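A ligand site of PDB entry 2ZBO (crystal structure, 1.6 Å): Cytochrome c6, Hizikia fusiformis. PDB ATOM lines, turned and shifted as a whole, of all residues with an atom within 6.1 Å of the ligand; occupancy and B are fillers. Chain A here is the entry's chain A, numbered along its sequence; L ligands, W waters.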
ATOM      1  N   VAL A   9      20.112  17.471  23.698  1.00  0.00           N
ATOM      2  CA  VAL A   9      20.534  18.646  22.903  1.00  0.00           C
ATOM      3  C   VAL A   9      20.000  18.503  21.472  1.00  0.00           C
ATOM      4  O   VAL A   9      19.475  19.464  20.899  1.00  0.00           O
ATOM      5  CB  VAL A   9      22.065  18.848  22.894  1.00  0.00           C
ATOM      6  CG1 VAL A   9      22.480  20.008  21.940  1.00  0.00           C
ATOM      7  CG2 VAL A   9      22.571  19.102  24.323  1.00  0.00           C
ATOM      8  N   PHE A  10      20.075  17.299  20.920  1.00  0.00           N
ATOM      9  CA  PHE A  10      19.568  17.051  19.567  1.00  0.00           C
ATOM     10  C   PHE A  10      18.055  17.313  19.464  1.00  0.00           C
ATOM     11  O   PHE A  10      17.596  17.993  18.547  1.00  0.00           O
ATOM     12  CB  PHE A  10      19.938  15.646  19.077  1.00  0.00           C
ATOM     13  CG  PHE A  10      19.729  15.428  17.608  1.00  0.00           C
ATOM     14  CD1 PHE A  10      20.753  15.631  16.699  1.00  0.00           C
ATOM     15  CD2 PHE A  10      18.483  14.991  17.139  1.00  0.00           C
ATOM     16  CE1 PHE A  10      20.544  15.440  15.320  1.00  0.00           C
ATOM     17  CE2 PHE A  10      18.267  14.784  15.770  1.00  0.00           C
ATOM     18  CZ  PHE A  10      19.292  15.007  14.874  1.00  0.00           C
ATOM     19  N   ASN A  13      17.349  21.155  19.648  1.00  0.00           N
ATOM     20  CA  ASN A  13      17.989  22.071  18.670  1.00  0.00           C
ATOM     21  C   ASN A  13      18.076  21.599  17.217  1.00  0.00           C
ATOM     22  O   ASN A  13      18.271  22.429  16.332  1.00  0.00           O
ATOM     23  CB  ASN A  13      19.423  22.410  19.122  1.00  0.00           C
ATOM     24  CG  ASN A  13      19.464  23.107  20.464  1.00  0.00           C
ATOM     25  OD1 ASN A  13      19.306  24.326  20.545  1.00  0.00           O
ATOM     26  ND2 ASN A  13      19.691  22.336  21.532  1.00  0.00           N
ATOM     27  N   CYS A  14      17.995  20.283  16.989  1.00  0.00           N
ATOM     28  CA  CYS A  14      18.348  19.726  15.690  1.00  0.00           C
ATOM     29  C   CYS A  14      17.228  18.926  15.042  1.00  0.00           C
ATOM     30  O   CYS A  14      17.209  18.757  13.810  1.00  0.00           O
ATOM     31  CB  CYS A  14      19.559  18.805  15.831  1.00  0.00           C
ATOM     32  SG  CYS A  14      20.915  19.408  16.933  1.00  0.00           S
ATOM     33  N   SER A  15      16.325  18.397  15.851  1.00  0.00           N
ATOM     34  CA  SER A  15      15.282  17.506  15.346  1.00  0.00           C
ATOM     35  C   SER A  15      14.366  18.195  14.331  1.00  0.00           C
ATOM     36  O   SER A  15      13.861  17.538  13.437  1.00  0.00           O
ATOM     37  CB  SER A  15      14.473  16.884  16.480  1.00  0.00           C
ATOM     38  OG  SER A  15      13.835  17.888  17.265  1.00  0.00           O
ATOM     39  N   ALA A  16      14.157  19.495  14.469  1.00  0.00           N
ATOM     40  CA  ALA A  16      13.328  20.243  13.521  1.00  0.00           C
ATOM     41  C   ALA A  16      13.769  20.011  12.077  1.00  0.00           C
ATOM     42  O   ALA A  16      12.924  19.880  11.192  1.00  0.00           O
ATOM     43  CB  ALA A  16      13.338  21.738  13.826  1.00  0.00           C
ATOM     44  N   CYS A  17      15.077  19.937  11.845  1.00  0.00           N
ATOM     45  CA  CYS A  17      15.601  19.741  10.488  1.00  0.00           C
ATOM     46  C   CYS A  17      16.179  18.356  10.246  1.00  0.00           C
ATOM     47  O   CYS A  17      16.312  17.961   9.090  1.00  0.00           O
ATOM     48  CB  CYS A  17      16.680  20.780  10.162  1.00  0.00           C
ATOM     49  SG  CYS A  17      16.062  22.488  10.179  1.00  0.00           S
ATOM     50  N   HIS A  18      16.533  17.644  11.302  1.00  0.00           N
ATOM     51  CA  HIS A  18      17.316  16.396  11.138  1.00  0.00           C
ATOM     52  C   HIS A  18      16.698  15.154  11.809  1.00  0.00           C
ATOM     53  O   HIS A  18      17.386  14.142  11.995  1.00  0.00           O
ATOM     54  CB  HIS A  18      18.761  16.593  11.675  1.00  0.00           C
ATOM     55  CG  HIS A  18      19.619  17.564  10.902  1.00  0.00           C
ATOM     56  ND1 HIS A  18      19.971  17.367   9.578  1.00  0.00           N
ATOM     57  CD2 HIS A  18      20.286  18.680  11.300  1.00  0.00           C
ATOM     58  CE1 HIS A  18      20.773  18.352   9.192  1.00  0.00           C
ATOM     59  NE2 HIS A  18      21.010  19.151  10.224  1.00  0.00           N
ATOM     60  N   ASN A  23      17.487  15.328   6.337  1.00  0.00           N
ATOM     61  CA  ASN A  23      17.758  16.751   6.278  1.00  0.00           C
ATOM     62  C   ASN A  23      16.635  17.394   5.492  1.00  0.00           C
ATOM     63  O   ASN A  23      16.504  17.151   4.301  1.00  0.00           O
ATOM     64  CB  ASN A  23      19.110  16.997   5.600  1.00  0.00           C
ATOM     65  CG  ASN A  23      19.541  18.456   5.647  1.00  0.00           C
ATOM     66  OD1 ASN A  23      18.714  19.373   5.550  1.00  0.00           O
ATOM     67  ND2 ASN A  23      20.857  18.672   5.749  1.00  0.00           N
ATOM     68  N   ILE A  25      15.984  20.536   4.621  1.00  0.00           N
ATOM     69  CA  ILE A  25      16.282  21.645   3.698  1.00  0.00           C
ATOM     70  C   ILE A  25      17.187  21.244   2.534  1.00  0.00           C
ATOM     71  O   ILE A  25      16.998  21.711   1.401  1.00  0.00           O
ATOM     72  CB  ILE A  25      16.828  22.884   4.448  1.00  0.00           C
ATOM     73  CG1 ILE A  25      15.747  23.445   5.382  1.00  0.00           C
ATOM     74  CG2 ILE A  25      17.289  23.974   3.474  1.00  0.00           C
ATOM     75  CD1 ILE A  25      16.188  24.682   6.192  1.00  0.00           C
ATOM     76  N   MET A  26      18.149  20.367   2.810  1.00  0.00           N
ATOM     77  CA  MET A  26      19.048  19.824   1.781  1.00  0.00           C
ATOM     78  C   MET A  26      19.042  18.309   1.917  1.00  0.00           C
ATOM     79  O   MET A  26      19.909  17.742   2.584  1.00  0.00           O
ATOM     80  CB  MET A  26      20.476  20.352   1.972  1.00  0.00           C
ATOM     81  CG  MET A  26      20.631  21.844   1.725  1.00  0.00           C
ATOM     82  SD  MET A  26      20.435  22.222  -0.041  1.00  0.00           S
ATOM     83  CE  MET A  26      22.072  21.843  -0.662  1.00  0.00           C
ATOM     84  N   GLU A  28      19.949  15.627   0.475  1.00  0.00           N
ATOM     85  CA  GLU A  28      21.117  14.750   0.250  1.00  0.00           C
ATOM     86  C   GLU A  28      22.115  14.779   1.406  1.00  0.00           C
ATOM     87  O   GLU A  28      22.902  13.834   1.595  1.00  0.00           O
ATOM     88  CB  GLU A  28      21.819  15.098  -1.057  1.00  0.00           C
ATOM     89  CG  GLU A  28      20.940  14.793  -2.249  1.00  0.00           C
ATOM     90  CD  GLU A  28      21.530  15.236  -3.567  1.00  0.00           C
ATOM     91  OE1 GLU A  28      22.749  15.015  -3.782  1.00  0.00           O
ATOM     92  OE2 GLU A  28      20.763  15.788  -4.397  1.00  0.00           O
ATOM     93  N   LYS A  29      22.088  15.851   2.199  1.00  0.00           N
ATOM     94  CA  LYS A  29      23.085  16.026   3.242  1.00  0.00           C
ATOM     95  C   LYS A  29      22.567  15.448   4.558  1.00  0.00           C
ATOM     96  O   LYS A  29      22.317  16.171   5.516  1.00  0.00           O
ATOM     97  CB  LYS A  29      23.430  17.513   3.419  1.00  0.00           C
ATOM     98  CG  LYS A  29      23.902  18.217   2.153  1.00  0.00           C
ATOM     99  CD  LYS A  29      25.322  17.860   1.801  1.00  0.00           C
ATOM    100  CE  LYS A  29      25.876  18.746   0.679  1.00  0.00           C
ATOM    101  NZ  LYS A  29      25.811  20.195   0.996  1.00  0.00           N
ATOM    102  N   THR A  30      22.408  14.119   4.589  1.00  0.00           N
ATOM    103  CA  THR A  30      21.862  13.430   5.757  1.00  0.00           C
ATOM    104  C   THR A  30      22.917  13.272   6.851  1.00  0.00           C
ATOM    105  O   THR A  30      24.089  13.642   6.672  1.00  0.00           O
ATOM    106  CB  THR A  30      21.385  12.017   5.408  1.00  0.00           C
ATOM    107  OG1 THR A  30      22.531  11.220   5.067  1.00  0.00           O
ATOM    108  CG2 THR A  30      20.373  12.023   4.237  1.00  0.00           C
ATOM    109  N   LEU A  31      22.482  12.707   7.977  1.00  0.00           N
ATOM    110  CA  LEU A  31      23.388  12.403   9.067  1.00  0.00           C
ATOM    111  C   LEU A  31      23.762  10.926   9.035  1.00  0.00           C
ATOM    112  O   LEU A  31      24.127  10.339  10.059  1.00  0.00           O
ATOM    113  CB  LEU A  31      22.761  12.817  10.414  1.00  0.00           C
ATOM    114  CG  LEU A  31      22.271  14.268  10.520  1.00  0.00           C
ATOM    115  CD1 LEU A  31      21.982  14.668  11.965  1.00  0.00           C
ATOM    116  CD2 LEU A  31      23.252  15.229   9.850  1.00  0.00           C
ATOM    117  N   GLN A  32      23.651  10.311   7.865  1.00  0.00           N
ATOM    118  CA  GLN A  32      24.080   8.911   7.689  1.00  0.00           C
ATOM    119  C   GLN A  32      25.562   8.849   7.316  1.00  0.00           C
ATOM    120  O   GLN A  32      26.094   9.805   6.770  1.00  0.00           O
ATOM    121  CB  GLN A  32      23.234   8.204   6.626  1.00  0.00           C
ATOM    122  CG  GLN A  32      21.707   8.140   6.918  1.00  0.00           C
ATOM    123  CD  GLN A  32      21.298   7.179   8.028  1.00  0.00           C
ATOM    124  OE1 GLN A  32      20.100   7.076   8.367  1.00  0.00           O
ATOM    125  NE2 GLN A  32      22.264   6.460   8.600  1.00  0.00           N
ATOM    126  N   ALA A  35      26.760   9.958   3.592  1.00  0.00           N
ATOM    127  CA  ALA A  35      26.681  11.391   3.312  1.00  0.00           C
ATOM    128  C   ALA A  35      27.694  12.159   4.163  1.00  0.00           C
ATOM    129  O   ALA A  35      28.354  13.060   3.669  1.00  0.00           O
ATOM    130  CB  ALA A  35      25.264  11.917   3.548  1.00  0.00           C
ATOM    131  N   LEU A  36      27.825  11.801   5.436  1.00  0.00           N
ATOM    132  CA  LEU A  36      28.801  12.486   6.287  1.00  0.00           C
ATOM    133  C   LEU A  36      30.197  12.349   5.694  1.00  0.00           C
ATOM    134  O   LEU A  36      30.907  13.339   5.523  1.00  0.00           O
ATOM    135  CB  LEU A  36      28.764  11.936   7.717  1.00  0.00           C
ATOM    136  CG  LEU A  36      27.549  12.275   8.569  1.00  0.00           C
ATOM    137  CD1 LEU A  36      27.551  11.452   9.839  1.00  0.00           C
ATOM    138  CD2 LEU A  36      27.461  13.778   8.895  1.00  0.00           C
ATOM    139  N   ASN A  39      31.002  14.393   2.642  1.00  0.00           N
ATOM    140  CA  ASN A  39      31.133  15.809   2.932  1.00  0.00           C
ATOM    141  C   ASN A  39      32.228  16.164   3.933  1.00  0.00           C
ATOM    142  O   ASN A  39      32.272  17.297   4.395  1.00  0.00           O
ATOM    143  CB  ASN A  39      29.770  16.370   3.380  1.00  0.00           C
ATOM    144  CG  ASN A  39      28.757  16.379   2.256  1.00  0.00           C
ATOM    145  OD1 ASN A  39      28.845  17.192   1.342  1.00  0.00           O
ATOM    146  ND2 ASN A  39      27.790  15.465   2.308  1.00  0.00           N
ATOM    147  N   MET A  41      32.433  15.236   6.905  1.00  0.00           N
ATOM    148  CA  MET A  41      31.715  15.523   8.132  1.00  0.00           C
ATOM    149  C   MET A  41      31.660  14.337   9.097  1.00  0.00           C
ATOM    150  O   MET A  41      31.038  14.408  10.158  1.00  0.00           O
ATOM    151  CB  MET A  41      30.284  16.021   7.817  1.00  0.00           C
ATOM    152  CG  MET A  41      30.256  17.397   7.156  1.00  0.00           C
ATOM    153  SD  MET A  41      30.855  18.685   8.289  1.00  0.00           S
ATOM    154  CE  MET A  41      29.647  18.575   9.577  1.00  0.00           C
ATOM    155  N   ILE A  47      31.914  17.943  12.917  1.00  0.00           N
ATOM    156  CA  ILE A  47      30.553  18.228  13.342  1.00  0.00           C
ATOM    157  C   ILE A  47      30.525  19.385  14.349  1.00  0.00           C
ATOM    158  O   ILE A  47      29.664  20.278  14.247  1.00  0.00           O
ATOM    159  CB  ILE A  47      29.848  16.972  13.900  1.00  0.00           C
ATOM    160  CG1 ILE A  47      29.697  15.958  12.759  1.00  0.00           C
ATOM    161  CG2 ILE A  47      28.450  17.329  14.504  1.00  0.00           C
ATOM    162  CD1 ILE A  47      29.305  14.561  13.218  1.00  0.00           C
ATOM    163  N   GLN A  50      30.859  22.754  12.492  1.00  0.00           N
ATOM    164  CA  GLN A  50      29.663  23.150  11.737  1.00  0.00           C
ATOM    165  C   GLN A  50      28.529  23.556  12.661  1.00  0.00           C
ATOM    166  O   GLN A  50      27.780  24.508  12.365  1.00  0.00           O
ATOM    167  CB  GLN A  50      29.205  22.007  10.836  1.00  0.00           C
ATOM    168  CG  GLN A  50      27.936  22.357  10.029  1.00  0.00           C
ATOM    169  CD  GLN A  50      27.930  21.799   8.611  1.00  0.00           C
ATOM    170  OE1 GLN A  50      26.857  21.399   8.108  1.00  0.00           O
ATOM    171  NE2 GLN A  50      29.079  21.799   7.947  1.00  0.00           N
ATOM    172  N   VAL A  51      28.364  22.830  13.770  1.00  0.00           N
ATOM    173  CA  VAL A  51      27.363  23.193  14.771  1.00  0.00           C
ATOM    174  C   VAL A  51      27.679  24.564  15.369  1.00  0.00           C
ATOM    175  O   VAL A  51      26.779  25.393  15.513  1.00  0.00           O
ATOM    176  CB  VAL A  51      27.233  22.129  15.864  1.00  0.00           C
ATOM    177  CG1 VAL A  51      26.410  22.630  17.052  1.00  0.00           C
ATOM    178  CG2 VAL A  51      26.618  20.852  15.273  1.00  0.00           C
ATOM    179  N   LYS A  55      26.714  26.529   8.559  1.00  0.00           N
ATOM    180  CA  LYS A  55      27.200  26.248   7.220  1.00  0.00           C
ATOM    181  C   LYS A  55      26.074  26.432   6.221  1.00  0.00           C
ATOM    182  O   LYS A  55      25.045  25.784   6.337  1.00  0.00           O
ATOM    183  CB  LYS A  55      27.718  24.812   7.141  1.00  0.00           C
ATOM    184  CG  LYS A  55      28.131  24.332   5.786  1.00  0.00           C
ATOM    185  CD  LYS A  55      29.440  24.940   5.375  1.00  0.00           C
ATOM    186  CE  LYS A  55      29.981  24.271   4.121  1.00  0.00           C
ATOM    187  NZ  LYS A  55      31.377  24.730   3.953  1.00  0.00           N
ATOM    188  N   ASN A  56      26.279  27.308   5.230  1.00  0.00           N
ATOM    189  CA  ASN A  56      25.264  27.565   4.208  1.00  0.00           C
ATOM    190  C   ASN A  56      23.908  27.833   4.888  1.00  0.00           C
ATOM    191  O   ASN A  56      23.829  28.738   5.718  1.00  0.00           O
ATOM    192  CB  ASN A  56      25.230  26.423   3.181  1.00  0.00           C
ATOM    193  CG  ASN A  56      26.541  26.309   2.408  1.00  0.00           C
ATOM    194  OD1 ASN A  56      27.237  27.299   2.224  1.00  0.00           O
ATOM    195  ND2 ASN A  56      26.880  25.098   1.947  1.00  0.00           N
ATOM    196  N   ALA A  57      22.863  27.075   4.566  1.00  0.00           N
ATOM    197  CA  ALA A  57      21.558  27.331   5.202  1.00  0.00           C
ATOM    198  C   ALA A  57      21.366  26.710   6.600  1.00  0.00           C
ATOM    199  O   ALA A  57      20.301  26.916   7.235  1.00  0.00           O
ATOM    200  CB  ALA A  57      20.410  26.950   4.264  1.00  0.00           C
ATOM    201  N   MET A  58      22.382  26.030   7.129  1.00  0.00           N
ATOM    202  CA  MET A  58      22.317  25.589   8.510  1.00  0.00           C
ATOM    203  C   MET A  58      22.779  26.710   9.438  1.00  0.00           C
ATOM    204  O   MET A  58      23.894  27.231   9.258  1.00  0.00           O
ATOM    205  CB  MET A  58      23.168  24.338   8.760  1.00  0.00           C
ATOM    206  CG  MET A  58      23.165  23.940  10.220  1.00  0.00           C
ATOM    207  SD  MET A  58      23.896  22.296  10.470  1.00  0.00           S
ATOM    208  CE  MET A  58      24.611  22.518  12.118  1.00  0.00           C
ATOM    209  N   PRO A  59      21.934  27.123  10.394  1.00  0.00           N
ATOM    210  CA  PRO A  59      22.349  28.204  11.302  1.00  0.00           C
ATOM    211  C   PRO A  59      23.455  27.799  12.270  1.00  0.00           C
ATOM    212  O   PRO A  59      23.757  26.592  12.389  1.00  0.00           O
ATOM    213  CB  PRO A  59      21.066  28.541  12.095  1.00  0.00           C
ATOM    214  CG  PRO A  59      20.145  27.408  11.871  1.00  0.00           C
ATOM    215  CD  PRO A  59      20.542  26.679  10.634  1.00  0.00           C
ATOM    216  N   PHE A  61      25.159  27.622  16.157  1.00  0.00           N
ATOM    217  CA  PHE A  61      24.708  27.320  17.508  1.00  0.00           C
ATOM    218  C   PHE A  61      25.711  27.720  18.599  1.00  0.00           C
ATOM    219  O   PHE A  61      25.449  27.497  19.788  1.00  0.00           O
ATOM    220  CB  PHE A  61      24.355  25.824  17.633  1.00  0.00           C
ATOM    221  CG  PHE A  61      23.156  25.409  16.833  1.00  0.00           C
ATOM    222  CD1 PHE A  61      23.278  25.177  15.455  1.00  0.00           C
ATOM    223  CD2 PHE A  61      21.914  25.263  17.426  1.00  0.00           C
ATOM    224  CE1 PHE A  61      22.175  24.806  14.679  1.00  0.00           C
ATOM    225  CE2 PHE A  61      20.784  24.902  16.666  1.00  0.00           C
ATOM    226  CZ  PHE A  61      20.920  24.670  15.302  1.00  0.00           C
ATOM    227  N   LEU A  65      24.586  27.178  22.541  1.00  0.00           N
ATOM    228  CA  LEU A  65      24.982  25.931  23.183  1.00  0.00           C
ATOM    229  C   LEU A  65      26.389  26.063  23.750  1.00  0.00           C
ATOM    230  O   LEU A  65      27.235  26.744  23.155  1.00  0.00           O
ATOM    231  CB  LEU A  65      24.937  24.765  22.169  1.00  0.00           C
ATOM    232  CG  LEU A  65      23.572  24.511  21.511  1.00  0.00           C
ATOM    233  CD1 LEU A  65      23.710  23.407  20.450  1.00  0.00           C
ATOM    234  CD2 LEU A  65      22.501  24.163  22.541  1.00  0.00           C
ATOM    235  N   VAL A  73      26.436  16.646  21.530  1.00  0.00           N
ATOM    236  CA  VAL A  73      25.534  16.433  20.392  1.00  0.00           C
ATOM    237  C   VAL A  73      26.262  15.839  19.180  1.00  0.00           C
ATOM    238  O   VAL A  73      25.697  14.993  18.470  1.00  0.00           O
ATOM    239  CB  VAL A  73      24.700  17.696  20.046  1.00  0.00           C
ATOM    240  CG1 VAL A  73      25.494  18.709  19.208  1.00  0.00           C
ATOM    241  CG2 VAL A  73      23.427  17.258  19.318  1.00  0.00           C
ATOM    242  N   ALA A  74      27.500  16.250  18.952  1.00  0.00           N
ATOM    243  CA  ALA A  74      28.315  15.688  17.867  1.00  0.00           C
ATOM    244  C   ALA A  74      28.561  14.207  18.092  1.00  0.00           C
ATOM    245  O   ALA A  74      28.488  13.404  17.144  1.00  0.00           O
ATOM    246  CB  ALA A  74      29.662  16.443  17.761  1.00  0.00           C
ATOM    247  N   VAL A  77      25.334  12.322  17.356  1.00  0.00           N
ATOM    248  CA  VAL A  77      25.152  12.185  15.898  1.00  0.00           C
ATOM    249  C   VAL A  77      25.954  10.998  15.358  1.00  0.00           C
ATOM    250  O   VAL A  77      25.419  10.182  14.595  1.00  0.00           O
ATOM    251  CB  VAL A  77      25.527  13.500  15.155  1.00  0.00           C
ATOM    252  CG1 VAL A  77      25.711  13.259  13.642  1.00  0.00           C
ATOM    253  CG2 VAL A  77      24.442  14.548  15.400  1.00  0.00           C
HETATM  254  C1  LIG L   1      24.067  19.803   7.621  1.00  0.00           C
HETATM  255  C2  LIG L   1      24.232  18.565  12.265  1.00  0.00           C
HETATM  256  C3  LIG L   1      20.803  21.840  13.231  1.00  0.00           C
HETATM  257  C4  LIG L   1      20.002  22.316   8.480  1.00  0.00           C
HETATM  258  C5  LIG L   1      24.425  19.159   8.779  1.00  0.00           C
HETATM  259  C6  LIG L   1      25.478  18.163   8.921  1.00  0.00           C
HETATM  260  C7  LIG L   1      25.503  17.847  10.224  1.00  0.00           C
HETATM  261  C8  LIG L   1      24.502  18.618  10.919  1.00  0.00           C
HETATM  262  C9  LIG L   1      26.427  16.837  10.949  1.00  0.00           C
HETATM  263  C10 LIG L   1      26.332  17.629   7.744  1.00  0.00           C
HETATM  264  C11 LIG L   1      25.505  16.590   6.962  1.00  0.00           C
HETATM  265  C12 LIG L   1      26.160  16.121   5.692  1.00  0.00           C
HETATM  266  O1  LIG L   1      27.040  16.831   5.133  1.00  0.00           O
HETATM  267  O2  LIG L   1      25.785  15.025   5.200  1.00  0.00           O
HETATM  268  C13 LIG L   1      23.337  19.365  12.943  1.00  0.00           C
HETATM  269  C14 LIG L   1      23.119  19.366  14.381  1.00  0.00           C
HETATM  270  C15 LIG L   1      22.172  20.275  14.669  1.00  0.00           C
HETATM  271  C16 LIG L   1      21.756  20.864  13.414  1.00  0.00           C
HETATM  272  C17 LIG L   1      23.876  18.460  15.388  1.00  0.00           C
HETATM  273  C18 LIG L   1      21.633  20.634  16.100  1.00  0.00           C
HETATM  274  C19 LIG L   1      22.509  21.382  16.850  1.00  0.00           C
HETATM  275  C20 LIG L   1      20.220  22.162  12.026  1.00  0.00           C
HETATM  276  C21 LIG L   1      18.927  22.812  11.866  1.00  0.00           C
HETATM  277  C22 LIG L   1      18.677  22.933  10.540  1.00  0.00           C
HETATM  278  C23 LIG L   1      19.825  22.387   9.836  1.00  0.00           C
HETATM  279  C24 LIG L   1      18.015  23.232  13.038  1.00  0.00           C
HETATM  280  C25 LIG L   1      17.374  23.499   9.905  1.00  0.00           C
HETATM  281  C26 LIG L   1      17.054  24.813  10.063  1.00  0.00           C
HETATM  282  C27 LIG L   1      21.107  21.817   7.823  1.00  0.00           C
HETATM  283  C28 LIG L   1      21.454  22.075   6.442  1.00  0.00           C
HETATM  284  C29 LIG L   1      22.714  21.298   6.183  1.00  0.00           C
HETATM  285  C30 LIG L   1      23.008  20.644   7.444  1.00  0.00           C
HETATM  286  C31 LIG L   1      20.701  22.954   5.415  1.00  0.00           C
HETATM  287  C32 LIG L   1      23.505  21.255   4.877  1.00  0.00           C
HETATM  288  C33 LIG L   1      24.463  22.466   4.856  1.00  0.00           C
HETATM  289  C34 LIG L   1      25.233  22.443   3.545  1.00  0.00           C
HETATM  290  O3  LIG L   1      26.241  21.689   3.424  1.00  0.00           O
HETATM  291  O4  LIG L   1      24.833  23.168   2.602  1.00  0.00           O
HETATM  292  N1  LIG L   1      23.854  19.413  10.003  1.00  0.00           N
HETATM  293  N2  LIG L   1      22.494  20.290  12.374  1.00  0.00           N
HETATM  294  N3  LIG L   1      20.728  21.905  10.766  1.00  0.00           N
HETATM  295  N4  LIG L   1      22.060  20.982   8.400  1.00  0.00           N
HETATM  296 FE1  LIG L   1      22.282  20.614  10.397  1.00  0.00          FE
HETATM  297  O   HOH W   1      25.340  22.773   0.028  1.00  0.00           O
HETATM  298  O   HOH W   2      22.524  24.755   2.874  1.00  0.00           O
HETATM  299  O   HOH W   3      28.328  21.734   1.896  1.00  0.00           O
HETATM  300  O   HOH W   4      27.144  20.025   5.347  1.00  0.00           O
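The side-chain amino group (NZ) of Lys 29 is in salt-bridge range of an oxygen (O3) of the ligand (2.9 Å). The side-chain sulfur (SG) of Cys 14 is covalently linked to a carbon (C18) of the ligand (1.6 Å). An oxygen (O2) of the ligand lies close to the backbone carbonyl oxygen (O) of Thr 30, at 2.6 Å. An iron atom (FE1) of the ligand is bound by the side-chain sulfur (SD) of Met 58. ND2 of Asn 56 sits at hydrogen-bond distance from O4 of the ligand, 2.9 Å away. NE2 of His 18 binds FE1 of the ligand (1.9 Å). ND2 of Asn 39 sits at hydrogen-bond distance from O1 of the ligand (3.2 Å). C25 of the ligand is covalently linked to SG of Cys 17 (1.7 Å).
The backbone carbonyl oxygen (O) of Lys 29 is in hydrogen-bond range of the side-chain amide nitrogen (ND2) of Asn 23 (2.9 Å). The side-chain amide oxygen (OD1) of Asn 23 sits at hydrogen-bond distance from the backbone NH (N) of Met 26 (3.0 Å). The backbone NH (N) of Phe 61 sits at hydrogen-bond distance from the backbone carbonyl oxygen (O) of Val 51. O of Val 9 is in hydrogen-bond range of ND2 of Asn 13. The backbone NH of Ile 25 lies within hydrogen-bond range of the side-chain amide oxygen of Asn 23, at 3.1 Å. The backbone NH (N) of Met 41 lies within hydrogen-bond range of the backbone carbonyl oxygen (O) of Leu 36, at 2.8 Å. O of Ala 35 sits at hydrogen-bond distance from ND2 of Asn 39, at 2.8 Å. OG1 of Thr 30 is in hydrogen-bond range of N of Gln 32, at 3.1 Å.
O of Asn 13 touches C24 of the ligand, at 3.4 Å. Asn 23 touches the ligand. Ile 25 touches the ligand. Met 26 touches the ligand. CD2 of Leu 31 touches C7 of the ligand, at 3.5 Å. Ala 35 touches the ligand. N of Leu 36 touches O2 of the ligand, at 3.8 Å. CG of Met 41 touches O1 of the ligand, 3.8 Å away. Ile 47 touches the ligand (CG1 to C9, 3.8 Å). OE1 of Gln 50 touches C1 of the ligand (3.3 Å). Val 51 touches the ligand. Lys 55 touches the ligand (O to C33, 3.7 Å). C of Ala 57 touches C31 of the ligand (3.99 Å). Pro 59 touches the ligand (CD to C26, 3.997 Å). CZ of Phe 61 touches C3 of the ligand, 3.5 Å away. Val 77 touches the ligand (CG2 to C17, 3.95 Å). Hydrophobic or aromatic side chains within 4 Å of the ligand: His 18, Ile 25, Met 26, Leu 31, Ala 35, Leu 36, Met 41, Ile 47, Val 51, Met 58, Pro 59, Phe 61 and Val 77. 24 residues have an atom within 4 Å of the ligand: Asn 13, Cys 14, Cys 17, His 18, Asn 23, Ile 25, Met 26, Lys 29, Thr 30, Leu 31, Ala 35, Leu 36, Asn 39, Met 41, Ile 47, Gln 50, Val 51, Lys 55, Asn 56, Ala 57, Met 58, Pro 59, Phe 61 and Val 77. The nearest printed residue that does not touch the ligand is Val 73 (4.1 Å).
Water W3 bridges O3 of the ligand (2.6 Å) and NZ of Lys 29 (3.1 Å). Water W1 lies within hydrogen-bond range of O4 of the ligand (2.7 Å), NZ of Lys 29 (2.8 Å) and ND2 of Asn 56 (3.4 Å). Water W4 bridges O3 of the ligand and OE1 of Gln 50. Water W2 lies within hydrogen-bond range of an oxygen (O4) of the ligand and the backbone NH of Ala 57.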
